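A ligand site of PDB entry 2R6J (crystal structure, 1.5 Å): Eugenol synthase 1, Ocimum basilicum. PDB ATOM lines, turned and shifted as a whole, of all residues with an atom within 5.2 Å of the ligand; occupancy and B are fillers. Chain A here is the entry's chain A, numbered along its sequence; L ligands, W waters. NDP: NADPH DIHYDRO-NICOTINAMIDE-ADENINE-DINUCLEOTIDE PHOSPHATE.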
ATOM      1  N   GLY A  18     -14.767  15.445  -9.177  1.00  0.00           N
ATOM      2  CA  GLY A  18     -14.860  15.388 -10.631  1.00  0.00           C
ATOM      3  C   GLY A  18     -14.200  14.143 -11.177  1.00  0.00           C
ATOM      4  O   GLY A  18     -13.795  14.093 -12.344  1.00  0.00           O
ATOM      5  N   THR A  20     -15.408  11.427 -12.128  1.00  0.00           N
ATOM      6  CA  THR A  20     -16.118  10.800 -13.249  1.00  0.00           C
ATOM      7  C   THR A  20     -15.897  11.595 -14.524  1.00  0.00           C
ATOM      8  O   THR A  20     -16.422  11.233 -15.578  1.00  0.00           O
ATOM      9  CB  THR A  20     -17.639  10.733 -13.009  1.00  0.00           C
ATOM     10  OG1 THR A  20     -18.160  12.057 -12.896  1.00  0.00           O
ATOM     11  CG2 THR A  20     -17.954   9.919 -11.757  1.00  0.00           C
ATOM     12  N   GLY A  21     -15.125  12.667 -14.433  1.00  0.00           N
ATOM     13  CA  GLY A  21     -14.890  13.528 -15.580  1.00  0.00           C
ATOM     14  C   GLY A  21     -13.991  13.016 -16.682  1.00  0.00           C
ATOM     15  O   GLY A  21     -13.361  11.965 -16.569  1.00  0.00           O
ATOM     16  N   TYR A  22     -13.919  13.797 -17.757  1.00  0.00           N
ATOM     17  CA  TYR A  22     -13.105  13.450 -18.906  1.00  0.00           C
ATOM     18  C   TYR A  22     -11.663  13.149 -18.514  1.00  0.00           C
ATOM     19  O   TYR A  22     -11.091  12.142 -18.930  1.00  0.00           O
ATOM     20  CB  TYR A  22     -13.130  14.566 -19.948  1.00  0.00           C
ATOM     21  CG  TYR A  22     -12.357  14.227 -21.188  1.00  0.00           C
ATOM     22  CD1 TYR A  22     -12.847  13.302 -22.120  1.00  0.00           C
ATOM     23  CD2 TYR A  22     -11.097  14.767 -21.409  1.00  0.00           C
ATOM     24  CE1 TYR A  22     -12.099  12.924 -23.229  1.00  0.00           C
ATOM     25  CE2 TYR A  22     -10.336  14.409 -22.524  1.00  0.00           C
ATOM     26  CZ  TYR A  22     -10.843  13.483 -23.427  1.00  0.00           C
ATOM     27  OH  TYR A  22     -10.083  13.097 -24.515  1.00  0.00           O
ATOM     28  N   ILE A  23     -11.070  14.019 -17.703  1.00  0.00           N
ATOM     29  CA  ILE A  23      -9.693  13.768 -17.263  1.00  0.00           C
ATOM     30  C   ILE A  23      -9.713  13.136 -15.868  1.00  0.00           C
ATOM     31  O   ILE A  23      -8.829  12.362 -15.518  1.00  0.00           O
ATOM     32  CB  ILE A  23      -8.826  15.078 -17.249  1.00  0.00           C
ATOM     33  CG1 ILE A  23      -7.340  14.700 -17.206  1.00  0.00           C
ATOM     34  CG2 ILE A  23      -9.171  15.952 -16.059  1.00  0.00           C
ATOM     35  CD1 ILE A  23      -6.827  14.052 -18.503  1.00  0.00           C
ATOM     36  N   GLY A  24     -10.732  13.459 -15.082  1.00  0.00           N
ATOM     37  CA  GLY A  24     -10.827  12.906 -13.749  1.00  0.00           C
ATOM     38  C   GLY A  24     -10.830  11.383 -13.671  1.00  0.00           C
ATOM     39  O   GLY A  24     -10.204  10.809 -12.773  1.00  0.00           O
ATOM     40  N   PHE A  41     -15.872  11.730  -5.146  1.00  0.00           N
ATOM     41  CA  PHE A  41     -17.056  12.514  -4.811  1.00  0.00           C
ATOM     42  C   PHE A  41     -17.838  12.700  -6.108  1.00  0.00           C
ATOM     43  O   PHE A  41     -17.264  13.039  -7.145  1.00  0.00           O
ATOM     44  CB  PHE A  41     -16.644  13.885  -4.247  1.00  0.00           C
ATOM     45  CG  PHE A  41     -17.736  14.573  -3.474  1.00  0.00           C
ATOM     46  CD1 PHE A  41     -18.025  14.188  -2.167  1.00  0.00           C
ATOM     47  CD2 PHE A  41     -18.455  15.618  -4.041  1.00  0.00           C
ATOM     48  CE1 PHE A  41     -19.030  14.827  -1.435  1.00  0.00           C
ATOM     49  CE2 PHE A  41     -19.459  16.270  -3.315  1.00  0.00           C
ATOM     50  CZ  PHE A  41     -19.744  15.864  -2.017  1.00  0.00           C
ATOM     51  N   THR A  42     -19.145  12.465  -6.063  1.00  0.00           N
ATOM     52  CA  THR A  42     -19.978  12.575  -7.246  1.00  0.00           C
ATOM     53  C   THR A  42     -21.392  13.046  -6.868  1.00  0.00           C
ATOM     54  O   THR A  42     -21.876  12.732  -5.779  1.00  0.00           O
ATOM     55  CB  THR A  42     -20.045  11.203  -7.976  1.00  0.00           C
ATOM     56  OG1 THR A  42     -20.891  11.303  -9.131  1.00  0.00           O
ATOM     57  CG2 THR A  42     -20.591  10.134  -7.031  1.00  0.00           C
ATOM     58  N   ARG A  43     -22.044  13.791  -7.756  1.00  0.00           N
ATOM     59  CA  ARG A  43     -23.387  14.291  -7.489  1.00  0.00           C
ATOM     60  C   ARG A  43     -24.394  13.145  -7.408  1.00  0.00           C
ATOM     61  O   ARG A  43     -24.217  12.102  -8.023  1.00  0.00           O
ATOM     62  CB  ARG A  43     -23.838  15.257  -8.592  1.00  0.00           C
ATOM     63  CG  ARG A  43     -23.201  16.649  -8.540  1.00  0.00           C
ATOM     64  CD  ARG A  43     -23.543  17.427  -9.796  1.00  0.00           C
ATOM     65  NE  ARG A  43     -23.025  16.746 -10.976  1.00  0.00           N
ATOM     66  CZ  ARG A  43     -23.400  17.016 -12.225  1.00  0.00           C
ATOM     67  NH1 ARG A  43     -22.879  16.331 -13.241  1.00  0.00           N
ATOM     68  NH2 ARG A  43     -24.307  17.962 -12.459  1.00  0.00           N
ATOM     69  N   SER A  46     -25.823  12.333 -10.950  1.00  0.00           N
ATOM     70  CA  SER A  46     -24.898  12.116 -12.052  1.00  0.00           C
ATOM     71  C   SER A  46     -25.344  10.957 -12.943  1.00  0.00           C
ATOM     72  O   SER A  46     -25.935   9.991 -12.463  1.00  0.00           O
ATOM     73  CB  SER A  46     -23.493  11.838 -11.529  1.00  0.00           C
ATOM     74  OG  SER A  46     -22.598  11.541 -12.589  1.00  0.00           O
ATOM     75  N   SER A  47     -25.067  11.067 -14.241  1.00  0.00           N
ATOM     76  CA  SER A  47     -25.434  10.017 -15.186  1.00  0.00           C
ATOM     77  C   SER A  47     -24.275   9.054 -15.390  1.00  0.00           C
ATOM     78  O   SER A  47     -24.369   8.127 -16.190  1.00  0.00           O
ATOM     79  CB  SER A  47     -25.815  10.642 -16.529  1.00  0.00           C
ATOM     80  OG  SER A  47     -24.728  11.327 -17.111  1.00  0.00           O
ATOM     81  N   LYS A  48     -23.189   9.265 -14.654  1.00  0.00           N
ATOM     82  CA  LYS A  48     -22.000   8.424 -14.739  1.00  0.00           C
ATOM     83  C   LYS A  48     -22.155   7.142 -13.904  1.00  0.00           C
ATOM     84  O   LYS A  48     -21.180   6.643 -13.343  1.00  0.00           O
ATOM     85  CB  LYS A  48     -20.776   9.207 -14.247  1.00  0.00           C
ATOM     86  CG  LYS A  48     -20.497  10.507 -15.003  1.00  0.00           C
ATOM     87  CD  LYS A  48     -19.993  10.250 -16.418  1.00  0.00           C
ATOM     88  CE  LYS A  48     -19.707  11.552 -17.153  1.00  0.00           C
ATOM     89  NZ  LYS A  48     -18.663  12.375 -16.484  1.00  0.00           N
ATOM     90  N   LEU A  67     -21.438  19.909  -3.589  1.00  0.00           N
ATOM     91  CA  LEU A  67     -20.371  20.748  -3.069  1.00  0.00           C
ATOM     92  C   LEU A  67     -20.884  21.711  -2.004  1.00  0.00           C
ATOM     93  O   LEU A  67     -20.113  22.233  -1.207  1.00  0.00           O
ATOM     94  CB  LEU A  67     -19.708  21.533  -4.206  1.00  0.00           C
ATOM     95  CG  LEU A  67     -18.991  20.651  -5.229  1.00  0.00           C
ATOM     96  CD1 LEU A  67     -18.449  21.504  -6.372  1.00  0.00           C
ATOM     97  CD2 LEU A  67     -17.862  19.892  -4.545  1.00  0.00           C
ATOM     98  N   ALA A  86     -10.749  17.893 -10.307  1.00  0.00           N
ATOM     99  CA  ALA A  86     -10.773  17.830 -11.763  1.00  0.00           C
ATOM    100  C   ALA A  86     -12.096  18.386 -12.258  1.00  0.00           C
ATOM    101  O   ALA A  86     -12.652  17.906 -13.253  1.00  0.00           O
ATOM    102  CB  ALA A  86     -10.587  16.394 -12.231  1.00  0.00           C
ATOM    103  N   LEU A  87     -12.617  19.394 -11.559  1.00  0.00           N
ATOM    104  CA  LEU A  87     -13.873  20.024 -11.948  1.00  0.00           C
ATOM    105  C   LEU A  87     -13.710  20.822 -13.243  1.00  0.00           C
ATOM    106  O   LEU A  87     -12.608  21.237 -13.595  1.00  0.00           O
ATOM    107  CB  LEU A  87     -14.377  20.938 -10.817  1.00  0.00           C
ATOM    108  CG  LEU A  87     -14.754  20.212  -9.521  1.00  0.00           C
ATOM    109  CD1 LEU A  87     -15.199  21.229  -8.480  1.00  0.00           C
ATOM    110  CD2 LEU A  87     -15.866  19.203  -9.788  1.00  0.00           C
ATOM    111  N   ALA A  88     -14.817  21.025 -13.945  1.00  0.00           N
ATOM    112  CA  ALA A  88     -14.823  21.746 -15.218  1.00  0.00           C
ATOM    113  C   ALA A  88     -14.816  23.272 -15.083  1.00  0.00           C
ATOM    114  O   ALA A  88     -15.011  23.814 -13.998  1.00  0.00           O
ATOM    115  CB  ALA A  88     -16.023  21.303 -16.054  1.00  0.00           C
ATOM    116  N   PHE A  89     -14.583  23.977 -16.196  1.00  0.00           N
ATOM    117  CA  PHE A  89     -14.520  25.431 -16.175  1.00  0.00           C
ATOM    118  C   PHE A  89     -15.701  26.124 -15.493  1.00  0.00           C
ATOM    119  O   PHE A  89     -15.496  27.075 -14.741  1.00  0.00           O
ATOM    120  CB  PHE A  89     -14.357  25.987 -17.593  1.00  0.00           C
ATOM    121  CG  PHE A  89     -12.939  26.430 -17.895  1.00  0.00           C
ATOM    122  CD1 PHE A  89     -12.244  25.888 -18.963  1.00  0.00           C
ATOM    123  CD2 PHE A  89     -12.321  27.386 -17.097  1.00  0.00           C
ATOM    124  CE1 PHE A  89     -10.928  26.280 -19.227  1.00  0.00           C
ATOM    125  CE2 PHE A  89     -11.004  27.788 -17.353  1.00  0.00           C
ATOM    126  CZ  PHE A  89     -10.312  27.222 -18.423  1.00  0.00           C
ATOM    127  N   GLN A  91     -17.330  25.301 -13.037  1.00  0.00           N
ATOM    128  CA  GLN A  91     -17.241  25.112 -11.593  1.00  0.00           C
ATOM    129  C   GLN A  91     -15.923  25.552 -10.964  1.00  0.00           C
ATOM    130  O   GLN A  91     -15.654  25.220  -9.820  1.00  0.00           O
ATOM    131  CB  GLN A  91     -17.472  23.637 -11.245  1.00  0.00           C
ATOM    132  CG  GLN A  91     -18.923  23.149 -11.266  1.00  0.00           C
ATOM    133  CD  GLN A  91     -19.544  23.149 -12.653  1.00  0.00           C
ATOM    134  OE1 GLN A  91     -19.070  22.436 -13.551  1.00  0.00           O
ATOM    135  NE2 GLN A  91     -20.598  23.935 -12.838  1.00  0.00           N
ATOM    136  N   ILE A  92     -15.099  26.308 -11.693  1.00  0.00           N
ATOM    137  CA  ILE A  92     -13.814  26.711 -11.118  1.00  0.00           C
ATOM    138  C   ILE A  92     -13.907  27.451  -9.787  1.00  0.00           C
ATOM    139  O   ILE A  92     -13.214  27.095  -8.826  1.00  0.00           O
ATOM    140  CB  ILE A  92     -12.987  27.554 -12.115  1.00  0.00           C
ATOM    141  CG1 ILE A  92     -12.623  26.705 -13.331  1.00  0.00           C
ATOM    142  CG2 ILE A  92     -11.696  28.079 -11.443  1.00  0.00           C
ATOM    143  CD1 ILE A  92     -11.860  25.408 -13.002  1.00  0.00           C
ATOM    144  N   SER A 114      -7.990  22.331 -10.011  1.00  0.00           N
ATOM    145  CA  SER A 114      -8.241  21.977 -11.393  1.00  0.00           C
ATOM    146  C   SER A 114      -7.589  22.938 -12.385  1.00  0.00           C
ATOM    147  O   SER A 114      -8.197  23.907 -12.825  1.00  0.00           O
ATOM    148  CB  SER A 114      -9.752  21.910 -11.664  1.00  0.00           C
ATOM    149  OG  SER A 114     -10.010  21.319 -12.934  1.00  0.00           O
ATOM    150  N   ASP A 115      -6.326  22.664 -12.699  1.00  0.00           N
ATOM    151  CA  ASP A 115      -5.573  23.449 -13.666  1.00  0.00           C
ATOM    152  C   ASP A 115      -5.539  22.535 -14.893  1.00  0.00           C
ATOM    153  O   ASP A 115      -6.429  22.601 -15.739  1.00  0.00           O
ATOM    154  CB  ASP A 115      -4.159  23.747 -13.145  1.00  0.00           C
ATOM    155  CG  ASP A 115      -4.134  24.918 -12.164  1.00  0.00           C
ATOM    156  OD1 ASP A 115      -4.949  25.842 -12.330  1.00  0.00           O
ATOM    157  OD2 ASP A 115      -3.296  24.907 -11.241  1.00  0.00           O
ATOM    158  N   PHE A 116      -4.537  21.677 -14.978  1.00  0.00           N
ATOM    159  CA  PHE A 116      -4.425  20.701 -16.055  1.00  0.00           C
ATOM    160  C   PHE A 116      -4.490  21.241 -17.494  1.00  0.00           C
ATOM    161  O   PHE A 116      -5.118  20.649 -18.370  1.00  0.00           O
ATOM    162  CB  PHE A 116      -5.489  19.614 -15.854  1.00  0.00           C
ATOM    163  CG  PHE A 116      -5.407  18.965 -14.497  1.00  0.00           C
ATOM    164  CD1 PHE A 116      -6.393  19.173 -13.544  1.00  0.00           C
ATOM    165  CD2 PHE A 116      -4.288  18.222 -14.138  1.00  0.00           C
ATOM    166  CE1 PHE A 116      -6.276  18.655 -12.253  1.00  0.00           C
ATOM    167  CE2 PHE A 116      -4.150  17.695 -12.862  1.00  0.00           C
ATOM    168  CZ  PHE A 116      -5.147  17.909 -11.916  1.00  0.00           C
ATOM    169  N   GLY A 117      -3.800  22.357 -17.732  1.00  0.00           N
ATOM    170  CA  GLY A 117      -3.779  22.937 -19.068  1.00  0.00           C
ATOM    171  C   GLY A 117      -2.572  23.847 -19.223  1.00  0.00           C
ATOM    172  O   GLY A 117      -1.449  23.439 -18.932  1.00  0.00           O
ATOM    173  N   LYS A 136      -8.864  30.464 -12.491  1.00  0.00           N
ATOM    174  CA  LYS A 136      -7.958  29.452 -11.973  1.00  0.00           C
ATOM    175  C   LYS A 136      -6.841  30.141 -11.176  1.00  0.00           C
ATOM    176  O   LYS A 136      -6.366  29.608 -10.181  1.00  0.00           O
ATOM    177  CB  LYS A 136      -7.373  28.597 -13.113  1.00  0.00           C
ATOM    178  CG  LYS A 136      -8.420  27.677 -13.755  1.00  0.00           C
ATOM    179  CD  LYS A 136      -7.801  26.725 -14.777  1.00  0.00           C
ATOM    180  CE  LYS A 136      -8.844  25.748 -15.304  1.00  0.00           C
ATOM    181  NZ  LYS A 136      -8.234  24.750 -16.259  1.00  0.00           N
ATOM    182  N   ASN A 156      -0.582  20.787 -20.221  1.00  0.00           N
ATOM    183  CA  ASN A 156      -0.522  21.153 -21.628  1.00  0.00           C
ATOM    184  C   ASN A 156      -1.735  20.540 -22.360  1.00  0.00           C
ATOM    185  O   ASN A 156      -2.745  20.266 -21.717  1.00  0.00           O
ATOM    186  CB  ASN A 156       0.826  20.771 -22.231  1.00  0.00           C
ATOM    187  CG  ASN A 156       1.931  21.736 -21.805  1.00  0.00           C
ATOM    188  OD1 ASN A 156       1.707  22.944 -21.707  1.00  0.00           O
ATOM    189  ND2 ASN A 156       3.124  21.211 -21.554  1.00  0.00           N
ATOM    190  N   CYS A 157      -1.650  20.305 -23.663  1.00  0.00           N
ATOM    191  CA  CYS A 157      -2.814  19.790 -24.392  1.00  0.00           C
ATOM    192  C   CYS A 157      -3.197  18.333 -24.169  1.00  0.00           C
ATOM    193  O   CYS A 157      -2.352  17.445 -24.192  1.00  0.00           O
ATOM    194  CB  CYS A 157      -2.618  20.002 -25.908  1.00  0.00           C
ATOM    195  SG  CYS A 157      -2.260  21.698 -26.434  1.00  0.00           S
ATOM    196  N   PHE A 158      -4.490  18.077 -23.963  1.00  0.00           N
ATOM    197  CA  PHE A 158      -4.983  16.700 -23.802  1.00  0.00           C
ATOM    198  C   PHE A 158      -4.859  16.140 -25.229  1.00  0.00           C
ATOM    199  O   PHE A 158      -5.516  16.629 -26.149  1.00  0.00           O
ATOM    200  CB  PHE A 158      -6.449  16.690 -23.343  1.00  0.00           C
ATOM    201  CG  PHE A 158      -6.657  17.011 -21.874  1.00  0.00           C
ATOM    202  CD1 PHE A 158      -5.583  17.335 -21.049  1.00  0.00           C
ATOM    203  CD2 PHE A 158      -7.937  16.985 -21.333  1.00  0.00           C
ATOM    204  CE1 PHE A 158      -5.788  17.645 -19.688  1.00  0.00           C
ATOM    205  CE2 PHE A 158      -8.160  17.285 -19.980  1.00  0.00           C
ATOM    206  CZ  PHE A 158      -7.074  17.616 -19.154  1.00  0.00           C
ATOM    207  N   TYR A 161      -7.998  14.382 -27.044  1.00  0.00           N
ATOM    208  CA  TYR A 161      -8.933  15.470 -27.228  1.00  0.00           C
ATOM    209  C   TYR A 161      -8.580  16.303 -28.450  1.00  0.00           C
ATOM    210  O   TYR A 161      -9.414  16.488 -29.348  1.00  0.00           O
ATOM    211  CB  TYR A 161      -8.939  16.363 -25.989  1.00  0.00           C
ATOM    212  CG  TYR A 161     -10.010  17.446 -25.988  1.00  0.00           C
ATOM    213  CD1 TYR A 161     -11.130  17.333 -25.165  1.00  0.00           C
ATOM    214  CD2 TYR A 161      -9.872  18.595 -26.758  1.00  0.00           C
ATOM    215  CE1 TYR A 161     -12.086  18.338 -25.109  1.00  0.00           C
ATOM    216  CE2 TYR A 161     -10.832  19.610 -26.715  1.00  0.00           C
ATOM    217  CZ  TYR A 161     -11.925  19.477 -25.880  1.00  0.00           C
ATOM    218  OH  TYR A 161     -12.868  20.487 -25.795  1.00  0.00           O
ATOM    219  N   PHE A 162      -7.344  16.801 -28.511  1.00  0.00           N
ATOM    220  CA  PHE A 162      -6.955  17.634 -29.641  1.00  0.00           C
ATOM    221  C   PHE A 162      -6.562  16.939 -30.941  1.00  0.00           C
ATOM    222  O   PHE A 162      -6.603  17.548 -32.004  1.00  0.00           O
ATOM    223  CB  PHE A 162      -5.909  18.656 -29.202  1.00  0.00           C
ATOM    224  CG  PHE A 162      -6.499  19.788 -28.411  1.00  0.00           C
ATOM    225  CD1 PHE A 162      -6.415  19.812 -27.031  1.00  0.00           C
ATOM    226  CD2 PHE A 162      -7.224  20.780 -29.061  1.00  0.00           C
ATOM    227  CE1 PHE A 162      -7.058  20.814 -26.295  1.00  0.00           C
ATOM    228  CE2 PHE A 162      -7.862  21.776 -28.354  1.00  0.00           C
ATOM    229  CZ  PHE A 162      -7.789  21.804 -26.967  1.00  0.00           C
ATOM    230  N   ALA A 316     -15.259  20.010 -24.265  1.00  0.00           N
ATOM    231  CA  ALA A 316     -15.278  20.534 -22.899  1.00  0.00           C
ATOM    232  C   ALA A 316     -16.495  21.424 -22.646  1.00  0.00           C
ATOM    233  O   ALA A 316     -17.057  22.003 -23.572  1.00  0.00           O
ATOM    234  CB  ALA A 316     -13.989  21.307 -22.621  1.00  0.00           C
ATOM    235  N   ALA A 317     -16.875  21.536 -21.374  1.00  0.00           N
ATOM    236  CA  ALA A 317     -18.015  22.353 -20.993  1.00  0.00           C
ATOM    237  C   ALA A 317     -17.574  23.781 -20.708  1.00  0.00           C
ATOM    238  O   ALA A 317     -16.547  24.002 -20.063  1.00  0.00           O
ATOM    239  CB  ALA A 317     -18.683  21.764 -19.752  1.00  0.00           C
HETATM  240  PA  NDP L   1     -15.824  17.446 -17.143  1.00  0.00           P
HETATM  241  O1A NDP L   1     -16.653  18.349 -17.971  1.00  0.00           O
HETATM  242  O2A NDP L   1     -15.610  16.041 -17.538  1.00  0.00           O
HETATM  243  O5B NDP L   1     -16.437  17.576 -15.668  1.00  0.00           O
HETATM  244  C5B NDP L   1     -15.786  16.913 -14.566  1.00  0.00           C
HETATM  245  C4B NDP L   1     -16.855  16.557 -13.569  1.00  0.00           C
HETATM  246  O4B NDP L   1     -17.573  17.689 -12.834  1.00  0.00           O
HETATM  247  C3B NDP L   1     -18.127  15.887 -14.078  1.00  0.00           C
HETATM  248  O3B NDP L   1     -17.831  14.551 -14.460  1.00  0.00           O
HETATM  249  C2B NDP L   1     -19.132  15.970 -12.925  1.00  0.00           C
HETATM  250  O2B NDP L   1     -19.028  14.860 -12.061  1.00  0.00           O
HETATM  251  C1B NDP L   1     -18.775  17.270 -12.218  1.00  0.00           C
HETATM  252  N9A NDP L   1     -19.776  18.330 -12.390  1.00  0.00           N
HETATM  253  C8A NDP L   1     -20.357  18.754 -13.594  1.00  0.00           C
HETATM  254  N7A NDP L   1     -21.232  19.725 -13.428  1.00  0.00           N
HETATM  255  C5A NDP L   1     -21.225  19.953 -12.092  1.00  0.00           C
HETATM  256  C6A NDP L   1     -21.950  20.864 -11.279  1.00  0.00           C
HETATM  257  N6A NDP L   1     -22.829  21.717 -11.799  1.00  0.00           N
HETATM  258  N1A NDP L   1     -21.702  20.847  -9.926  1.00  0.00           N
HETATM  259  C2A NDP L   1     -20.801  19.971  -9.401  1.00  0.00           C
HETATM  260  N3A NDP L   1     -20.063  19.055 -10.086  1.00  0.00           N
HETATM  261  C4A NDP L   1     -20.331  19.106 -11.436  1.00  0.00           C
HETATM  262  O3  NDP L   1     -14.393  18.202 -16.896  1.00  0.00           O
HETATM  263  PN  NDP L   1     -13.104  18.078 -17.850  1.00  0.00           P
HETATM  264  O1N NDP L   1     -13.476  18.274 -19.277  1.00  0.00           O
HETATM  265  O2N NDP L   1     -12.451  16.786 -17.513  1.00  0.00           O
HETATM  266  O5D NDP L   1     -12.153  19.260 -17.352  1.00  0.00           O
HETATM  267  C5D NDP L   1     -11.416  19.157 -16.118  1.00  0.00           C
HETATM  268  C4D NDP L   1     -10.214  20.063 -16.146  1.00  0.00           C
HETATM  269  O4D NDP L   1      -9.399  19.728 -17.301  1.00  0.00           O
HETATM  270  C3D NDP L   1     -10.542  21.574 -16.188  1.00  0.00           C
HETATM  271  O3D NDP L   1      -9.669  22.328 -15.375  1.00  0.00           O
HETATM  272  C2D NDP L   1     -10.411  21.836 -17.655  1.00  0.00           C
HETATM  273  O2D NDP L   1     -10.157  23.208 -17.886  1.00  0.00           O
HETATM  274  C1D NDP L   1      -9.291  20.931 -18.080  1.00  0.00           C
HETATM  275  N1N NDP L   1      -9.274  20.671 -19.534  1.00  0.00           N
HETATM  276  C2N NDP L   1      -8.057  20.856 -20.165  1.00  0.00           C
HETATM  277  C3N NDP L   1      -7.888  20.463 -21.491  1.00  0.00           C
HETATM  278  C7N NDP L   1      -6.512  20.415 -22.126  1.00  0.00           C
HETATM  279  O7N NDP L   1      -6.403  20.100 -23.308  1.00  0.00           O
HETATM  280  N7N NDP L   1      -5.464  20.717 -21.352  1.00  0.00           N
HETATM  281  C4N NDP L   1      -9.031  20.055 -22.239  1.00  0.00           C
HETATM  282  C5N NDP L   1     -10.257  19.828 -21.583  1.00  0.00           C
HETATM  283  C6N NDP L   1     -10.356  20.082 -20.207  1.00  0.00           C
HETATM  284  P2B NDP L   1     -20.314  14.133 -11.417  1.00  0.00           P
HETATM  285  O1X NDP L   1     -21.326  13.910 -12.525  1.00  0.00           O
HETATM  286  O2X NDP L   1     -19.681  12.897 -10.840  1.00  0.00           O
HETATM  287  O3X NDP L   1     -20.829  15.071 -10.341  1.00  0.00           O
HETATM  288  O   HOH W   1     -22.167  19.605  -6.377  1.00  0.00           O
HETATM  289  O   HOH W   2     -12.606  15.709 -15.052  1.00  0.00           O
HETATM  290  O   HOH W   3     -19.210  19.124 -16.886  1.00  0.00           O
HETATM  291  O   HOH W   4     -17.541  14.395 -18.421  1.00  0.00           O
HETATM  292  O   HOH W   5     -17.330  20.511 -12.859  1.00  0.00           O
HETATM  293  O   HOH W   6     -19.367  16.549  -8.575  1.00  0.00           O
HETATM  294  O   HOH W   7     -11.968  22.972 -20.266  1.00  0.00           O
HETATM  295  O   HOH W   8     -20.881  13.889 -15.223  1.00  0.00           O
HETATM  296  O   HOH W   9     -13.336  17.533 -21.916  1.00  0.00           O
HETATM  297  O   HOH W  10     -15.337  20.230 -19.376  1.00  0.00           O
HETATM  298  O   HOH W  11     -17.809  17.364 -20.310  1.00  0.00           O
HETATM  299  O   HOH W  12     -17.045  12.910  -9.966  1.00  0.00           O
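The backbone carbonyl oxygen (O) of Leu 87 lies within hydrogen-bond range of the side-chain hydroxyl (OG) of Ser 114 (2.7 Å).
The backbone NH (N) of Lys 48 sits at hydrogen-bond distance from the side-chain hydroxyl (OG) of Ser 46 (3.1 Å).
The backbone carbonyl oxygen (O) of Thr 20 lies within hydrogen-bond range of the side-chain amino group (NZ) of Lys 48.
The backbone carbonyl oxygen (O) of Gly 117 sits at hydrogen-bond distance from the backbone NH (N) of Asn 156 (3.1 Å).
The side-chain amino group (NZ) of Lys 136 is in hydrogen-bond range of the backbone carbonyl oxygen (O) of Asp 115, 2.9 Å away.
Water W4 bridges O2A of the ligand (2.7 Å) and NZ of Lys 48 (3.0 Å).
Water W2 lies within hydrogen-bond range of O2N of the ligand (2.7 Å), O of Ala 86 (2.8 Å), N of Gly 24 (2.9 Å), O of Gly 18 (3.4 Å) and N of Ile 23 (3.5 Å).
Water W10 lies within hydrogen-bond range of an oxygen (O1A) of the ligand (2.7 Å) and the backbone NH of Ala 317 (2.8 Å).
Water W8 lies within hydrogen-bond range of O1X of the ligand (2.7 Å) and NZ of Lys 48 (3.0 Å).
Water W12 lies within hydrogen-bond range of O2X of the ligand (2.8 Å), O of Phe 41 (2.8 Å), N of Thr 20 (3.1 Å) and N of Gly 18 (3.5 Å).
Water W5 lies within hydrogen-bond range of OE1 of Gln 91 (2.7 Å), N of Ala 88 (2.8 Å) and O4B of the ligand (2.8 Å).
The side-chain hydroxyl (OG1) of Thr 42 lies within hydrogen-bond range of an oxygen (O2X) of the ligand (2.6 Å).
An oxygen (O3D) of the ligand sits at hydrogen-bond distance from the backbone carbonyl oxygen of Ser 114 (3.3 Å).
The side-chain hydroxyl (OG) of Ser 114 sits at hydrogen-bond distance from an oxygen (O3D) of the ligand (2.7 Å).
OG of Ser 46 lies within hydrogen-bond range of O1X of the ligand.
OG1 of Thr 20 lies within hydrogen-bond range of O2X of the ligand (2.7 Å).
N7N of the ligand is in hydrogen-bond range of O of Asn 156 (2.8 Å).
O2A of the ligand sits at hydrogen-bond distance from N of Tyr 22 (2.8 Å).
The backbone NH of Arg 43 sits at hydrogen-bond distance from an oxygen (O3X) of the ligand, at 3.1 Å.
The guanidinium group (NE) of Arg 43 lies within salt-bridge range of an oxygen (O3X) of the ligand, 2.8 Å away.
O7N of the ligand lies within hydrogen-bond range of N of Phe 158, at 2.9 Å.
An oxygen (O3D) of the ligand is in hydrogen-bond range of the side-chain amino group (NZ) of Lys 136 (3.0 Å).
A nitrogen (N7N) of the ligand sits at hydrogen-bond distance from the backbone carbonyl oxygen (O) of Phe 116.
An oxygen (O3B) of the ligand lies within hydrogen-bond range of the side-chain amino group (NZ) of Lys 48.
N of Ile 23 sits at hydrogen-bond distance from O2N of the ligand (3.1 Å).
The backbone NH of Gly 21 lies within hydrogen-bond range of an oxygen (O3B) of the ligand.
The backbone carbonyl oxygen of Asp 115 lies within hydrogen-bond range of an oxygen (O3D) of the ligand (3.3 Å).
The side-chain amide nitrogen (NE2) of Gln 91 sits close to a nitrogen (N6A) of the ligand (3.3 Å).
CA of Gly 18 touches C4B of the ligand, 3.7 Å away.
O of Ala 86 touches C5D of the ligand, at 3.4 Å.
Leu 87 touches the ligand (O to C3D, 3.3 Å).
CB of Ala 88 touches O1A of the ligand (3.6 Å).
CE1 of Phe 89 touches O2D of the ligand (3.4 Å).
Gly 117 touches the ligand (CA to N7N, 3.6 Å).
Cys 157 touches the ligand.
Phe 162 touches the ligand.
Of the 31 residues printed, 23 come within 4 Å of the ligand.
Along chain A the residues within 4 Å of the ligand span positions 18 to 162.
The nearest printed residue that does not touch the ligand is Leu 67 (4.1 Å).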
